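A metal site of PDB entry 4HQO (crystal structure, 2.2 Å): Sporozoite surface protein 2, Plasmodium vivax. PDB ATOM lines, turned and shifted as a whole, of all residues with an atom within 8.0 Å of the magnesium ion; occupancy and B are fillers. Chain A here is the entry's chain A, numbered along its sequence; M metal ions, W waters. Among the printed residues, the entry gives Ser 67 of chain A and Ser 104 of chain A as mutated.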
ATOM      1  N   ASP A  26     -21.627  22.910  23.995  1.00  0.00           N
ATOM      2  CA  ASP A  26     -20.567  23.906  24.204  1.00  0.00           C
ATOM      3  C   ASP A  26     -19.360  23.538  23.337  1.00  0.00           C
ATOM      4  O   ASP A  26     -18.721  22.513  23.570  1.00  0.00           O
ATOM      5  CB  ASP A  26     -20.177  23.866  25.691  1.00  0.00           C
ATOM      6  CG  ASP A  26     -19.276  25.020  26.113  1.00  0.00           C
ATOM      7  OD1 ASP A  26     -18.542  25.593  25.275  1.00  0.00           O
ATOM      8  OD2 ASP A  26     -19.317  25.346  27.325  1.00  0.00           O
ATOM      9  N   GLY A  27     -19.039  24.371  22.354  1.00  0.00           N
ATOM     10  CA  GLY A  27     -17.857  24.138  21.510  1.00  0.00           C
ATOM     11  C   GLY A  27     -16.777  25.189  21.680  1.00  0.00           C
ATOM     12  O   GLY A  27     -15.961  25.428  20.785  1.00  0.00           O
ATOM     13  N   SER A  28     -16.761  25.843  22.850  1.00  0.00           N
ATOM     14  CA  SER A  28     -15.842  26.935  23.134  1.00  0.00           C
ATOM     15  C   SER A  28     -14.410  26.459  23.375  1.00  0.00           C
ATOM     16  O   SER A  28     -14.147  25.270  23.580  1.00  0.00           O
ATOM     17  CB  SER A  28     -16.322  27.723  24.356  1.00  0.00           C
ATOM     18  OG  SER A  28     -16.141  26.978  25.550  1.00  0.00           O
ATOM     19  N   GLY A  29     -13.479  27.409  23.396  1.00  0.00           N
ATOM     20  CA  GLY A  29     -12.076  27.116  23.614  1.00  0.00           C
ATOM     21  C   GLY A  29     -11.768  26.421  24.927  1.00  0.00           C
ATOM     22  O   GLY A  29     -10.888  25.579  24.986  1.00  0.00           O
ATOM     23  N   SER A  30     -12.487  26.776  26.005  1.00  0.00           N
ATOM     24  CA  SER A  30     -12.232  26.151  27.293  1.00  0.00           C
ATOM     25  C   SER A  30     -12.562  24.644  27.312  1.00  0.00           C
ATOM     26  O   SER A  30     -12.023  23.894  28.134  1.00  0.00           O
ATOM     27  CB  SER A  30     -12.955  26.874  28.425  1.00  0.00           C
ATOM     28  OG  SER A  30     -14.357  26.868  28.215  1.00  0.00           O
ATOM     29  N   ILE A  31     -13.421  24.197  26.417  1.00  0.00           N
ATOM     30  CA  ILE A  31     -13.693  22.769  26.332  1.00  0.00           C
ATOM     31  C   ILE A  31     -12.410  22.013  25.975  1.00  0.00           C
ATOM     32  O   ILE A  31     -12.002  21.077  26.657  1.00  0.00           O
ATOM     33  CB  ILE A  31     -14.801  22.481  25.312  1.00  0.00           C
ATOM     34  CG1 ILE A  31     -16.087  23.168  25.754  1.00  0.00           C
ATOM     35  CG2 ILE A  31     -15.017  20.974  25.161  1.00  0.00           C
ATOM     36  CD1 ILE A  31     -16.520  22.811  27.163  1.00  0.00           C
ATOM     37  N   GLY A  32     -11.738  22.465  24.917  1.00  0.00           N
ATOM     38  CA  GLY A  32     -10.467  21.875  24.546  1.00  0.00           C
ATOM     39  C   GLY A  32     -10.603  20.768  23.522  1.00  0.00           C
ATOM     40  O   GLY A  32     -11.520  19.957  23.582  1.00  0.00           O
ATOM     41  N   PHE A  65     -22.610  26.045  20.427  1.00  0.00           N
ATOM     42  CA  PHE A  65     -22.305  27.411  20.840  1.00  0.00           C
ATOM     43  C   PHE A  65     -20.854  27.608  21.266  1.00  0.00           C
ATOM     44  O   PHE A  65     -20.249  26.759  21.910  1.00  0.00           O
ATOM     45  CB  PHE A  65     -23.284  27.926  21.896  1.00  0.00           C
ATOM     46  CG  PHE A  65     -23.257  27.170  23.198  1.00  0.00           C
ATOM     47  CD1 PHE A  65     -24.024  26.031  23.381  1.00  0.00           C
ATOM     48  CD2 PHE A  65     -22.475  27.632  24.256  1.00  0.00           C
ATOM     49  CE1 PHE A  65     -24.020  25.349  24.588  1.00  0.00           C
ATOM     50  CE2 PHE A  65     -22.465  26.950  25.484  1.00  0.00           C
ATOM     51  CZ  PHE A  65     -23.238  25.810  25.646  1.00  0.00           C
ATOM     52  N   GLY A  66     -20.306  28.747  20.872  1.00  0.00           N
ATOM     53  CA  GLY A  66     -18.928  29.090  21.153  1.00  0.00           C
ATOM     54  C   GLY A  66     -18.865  30.592  21.062  1.00  0.00           C
ATOM     55  O   GLY A  66     -19.650  31.263  21.720  1.00  0.00           O
ATOM     56  N   SER A  67     -17.956  31.117  20.245  1.00  0.00           N
ATOM     57  CA  SER A  67     -17.901  32.562  20.006  1.00  0.00           C
ATOM     58  C   SER A  67     -19.196  33.018  19.358  1.00  0.00           C
ATOM     59  O   SER A  67     -19.660  34.140  19.576  1.00  0.00           O
ATOM     60  CB  SER A  67     -16.724  32.922  19.072  1.00  0.00           C
ATOM     61  OG  SER A  67     -15.498  32.933  19.784  1.00  0.00           O
ATOM     62  N   TYR A 100     -13.011  26.420  19.865  1.00  0.00           N
ATOM     63  CA  TYR A 100     -12.293  27.672  19.981  1.00  0.00           C
ATOM     64  C   TYR A 100     -13.253  28.737  20.476  1.00  0.00           C
ATOM     65  O   TYR A 100     -14.479  28.594  20.372  1.00  0.00           O
ATOM     66  CB  TYR A 100     -11.733  28.101  18.605  1.00  0.00           C
ATOM     67  CG  TYR A 100     -12.804  28.657  17.685  1.00  0.00           C
ATOM     68  CD1 TYR A 100     -13.593  27.793  16.911  1.00  0.00           C
ATOM     69  CD2 TYR A 100     -13.050  30.033  17.597  1.00  0.00           C
ATOM     70  CE1 TYR A 100     -14.599  28.295  16.068  1.00  0.00           C
ATOM     71  CE2 TYR A 100     -14.049  30.535  16.775  1.00  0.00           C
ATOM     72  CZ  TYR A 100     -14.815  29.670  16.003  1.00  0.00           C
ATOM     73  OH  TYR A 100     -15.795  30.167  15.171  1.00  0.00           O
ATOM     74  N   GLY A 101     -12.709  29.821  21.012  1.00  0.00           N
ATOM     75  CA  GLY A 101     -13.488  31.000  21.274  1.00  0.00           C
ATOM     76  C   GLY A 101     -14.173  31.051  22.621  1.00  0.00           C
ATOM     77  O   GLY A 101     -13.921  30.235  23.505  1.00  0.00           O
ATOM     78  N   THR A 102     -15.042  32.033  22.766  1.00  0.00           N
ATOM     79  CA  THR A 102     -15.757  32.244  24.007  1.00  0.00           C
ATOM     80  C   THR A 102     -17.026  31.361  24.032  1.00  0.00           C
ATOM     81  O   THR A 102     -17.127  30.414  23.261  1.00  0.00           O
ATOM     82  CB  THR A 102     -16.059  33.741  24.202  1.00  0.00           C
ATOM     83  OG1 THR A 102     -16.686  34.252  23.021  1.00  0.00           O
ATOM     84  CG2 THR A 102     -14.733  34.532  24.430  1.00  0.00           C
ATOM     85  N   THR A 103     -17.966  31.656  24.928  1.00  0.00           N
ATOM     86  CA  THR A 103     -19.045  30.719  25.243  1.00  0.00           C
ATOM     87  C   THR A 103     -20.430  31.375  25.237  1.00  0.00           C
ATOM     88  O   THR A 103     -20.912  31.828  26.279  1.00  0.00           O
ATOM     89  CB  THR A 103     -18.798  30.070  26.620  1.00  0.00           C
ATOM     90  OG1 THR A 103     -17.417  29.698  26.731  1.00  0.00           O
ATOM     91  CG2 THR A 103     -19.684  28.852  26.823  1.00  0.00           C
ATOM     92  N   SER A 104     -21.060  31.437  24.071  1.00  0.00           N
ATOM     93  CA  SER A 104     -22.362  32.060  23.914  1.00  0.00           C
ATOM     94  C   SER A 104     -23.516  31.212  24.467  1.00  0.00           C
ATOM     95  O   SER A 104     -24.423  30.803  23.734  1.00  0.00           O
ATOM     96  CB  SER A 104     -22.613  32.356  22.435  1.00  0.00           C
ATOM     97  OG  SER A 104     -21.711  33.342  21.966  1.00  0.00           O
ATOM     98  N   MET A 105     -23.489  30.954  25.771  1.00  0.00           N
ATOM     99  CA  MET A 105     -24.448  30.012  26.349  1.00  0.00           C
ATOM    100  C   MET A 105     -25.862  30.605  26.418  1.00  0.00           C
ATOM    101  O   MET A 105     -26.842  29.919  26.160  1.00  0.00           O
ATOM    102  CB  MET A 105     -23.986  29.568  27.744  1.00  0.00           C
ATOM    103  CG  MET A 105     -24.919  28.589  28.411  1.00  0.00           C
ATOM    104  SD  MET A 105     -24.426  28.232  30.107  1.00  0.00           S
ATOM    105  CE  MET A 105     -22.806  27.515  29.824  1.00  0.00           C
ATOM    106  N   THR A 133     -21.931  21.413  28.857  1.00  0.00           N
ATOM    107  CA  THR A 133     -21.012  22.528  29.056  1.00  0.00           C
ATOM    108  C   THR A 133     -20.025  22.291  30.208  1.00  0.00           C
ATOM    109  O   THR A 133     -20.258  21.420  31.050  1.00  0.00           O
ATOM    110  CB  THR A 133     -21.818  23.831  29.300  1.00  0.00           C
ATOM    111  OG1 THR A 133     -20.919  24.954  29.379  1.00  0.00           O
ATOM    112  CG2 THR A 133     -22.629  23.724  30.603  1.00  0.00           C
ATOM    113  N   ASP A 134     -18.933  23.048  30.227  1.00  0.00           N
ATOM    114  CA  ASP A 134     -18.045  23.099  31.394  1.00  0.00           C
ATOM    115  C   ASP A 134     -18.508  24.164  32.394  1.00  0.00           C
ATOM    116  O   ASP A 134     -17.918  24.329  33.457  1.00  0.00           O
ATOM    117  CB  ASP A 134     -16.581  23.357  30.986  1.00  0.00           C
ATOM    118  CG  ASP A 134     -16.370  24.726  30.337  1.00  0.00           C
ATOM    119  OD1 ASP A 134     -17.337  25.521  30.217  1.00  0.00           O
ATOM    120  OD2 ASP A 134     -15.222  24.998  29.949  1.00  0.00           O
ATOM    121  N   GLY A 135     -19.539  24.913  32.022  1.00  0.00           N
ATOM    122  CA  GLY A 135     -20.172  25.815  32.969  1.00  0.00           C
ATOM    123  C   GLY A 135     -19.453  27.139  33.160  1.00  0.00           C
ATOM    124  O   GLY A 135     -19.475  27.697  34.258  1.00  0.00           O
ATOM    125  N   VAL A 136     -18.826  27.635  32.084  1.00  0.00           N
ATOM    126  CA  VAL A 136     -18.185  28.953  32.098  1.00  0.00           C
ATOM    127  C   VAL A 136     -18.743  29.818  30.957  1.00  0.00           C
ATOM    128  O   VAL A 136     -18.111  29.951  29.901  1.00  0.00           O
ATOM    129  CB  VAL A 136     -16.644  28.833  31.951  1.00  0.00           C
ATOM    130  CG1 VAL A 136     -15.973  30.154  32.318  1.00  0.00           C
ATOM    131  CG2 VAL A 136     -16.113  27.724  32.850  1.00  0.00           C
ATOM    132  N   PRO A 137     -19.950  30.377  31.151  1.00  0.00           N
ATOM    133  CA  PRO A 137     -20.558  31.180  30.083  1.00  0.00           C
ATOM    134  C   PRO A 137     -19.944  32.576  29.994  1.00  0.00           C
ATOM    135  O   PRO A 137     -19.217  33.006  30.900  1.00  0.00           O
ATOM    136  CB  PRO A 137     -22.033  31.272  30.515  1.00  0.00           C
ATOM    137  CG  PRO A 137     -21.964  31.214  32.018  1.00  0.00           C
ATOM    138  CD  PRO A 137     -20.844  30.225  32.308  1.00  0.00           C
ATOM    139  N   ASN A 138     -20.245  33.279  28.900  1.00  0.00           N
ATOM    140  CA  ASN A 138     -19.800  34.657  28.739  1.00  0.00           C
ATOM    141  C   ASN A 138     -20.408  35.580  29.772  1.00  0.00           C
ATOM    142  O   ASN A 138     -19.806  36.592  30.123  1.00  0.00           O
ATOM    143  CB  ASN A 138     -20.118  35.174  27.334  1.00  0.00           C
ATOM    144  CG  ASN A 138     -19.215  34.567  26.261  1.00  0.00           C
ATOM    145  OD1 ASN A 138     -18.212  33.921  26.567  1.00  0.00           O
ATOM    146  ND2 ASN A 138     -19.572  34.780  24.999  1.00  0.00           N
ATOM    147  N   GLY A 165     -11.911  21.509  32.172  1.00  0.00           N
ATOM    148  CA  GLY A 165     -11.993  22.238  33.436  1.00  0.00           C
ATOM    149  C   GLY A 165     -13.409  22.667  33.769  1.00  0.00           C
ATOM    150  O   GLY A 165     -13.813  23.802  33.497  1.00  0.00           O
HETATM  151 MG    MG M   1     -15.757  28.386  27.322  1.00  0.00          MG
HETATM  152  O   HOH W   1     -14.022  29.327  26.380  1.00  0.00           O
HETATM  153  O   HOH W   2     -17.389  27.236  28.145  1.00  0.00           O
HETATM  154  O   HOH W   3     -15.380  29.920  28.753  1.00  0.00           O
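OG1 of Thr 103 sits close to O of Val 136 (3.3 Å). The side-chain amide oxygen of Asn 138 sits at hydrogen-bond distance from the backbone NH of Thr 103 (2.8 Å). The side-chain hydroxyl of Ser 30 sits close to the side-chain carboxylate of Asp 134 (2.7 Å). N of Ser 28 lies within hydrogen-bond range of OD1 of Asp 26. The side-chain carboxylate (OD1) of Asp 134 lies within hydrogen-bond range of the backbone NH (N) of Val 136 (3.2 Å).
Residues that only touch the magnesium ion: Val 136. Four residues have an atom within 4 Å of the magnesium ion: Ser 28, Ser 30, Thr 103 and Val 136. The nearest printed residue that does not touch the magnesium ion is Asp 134 (4.3 Å).
Water W1 lies within hydrogen-bond range of the backbone NH of Ser 30 (3.0 Å) and the backbone carbonyl oxygen of Gly 101 (3.0 Å).
The magnesium ion is bound by water W3, 2.1 Å away. Water W2 binds the magnesium ion, at 2.2 Å. Water W1 binds the magnesium ion, at 2.2 Å. OG1 of Thr 103 is bound to the magnesium ion (2.2 Å). The side-chain hydroxyl (OG) of Ser 30 binds the magnesium ion (2.2 Å). The magnesium ion is bound by OG of Ser 28.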
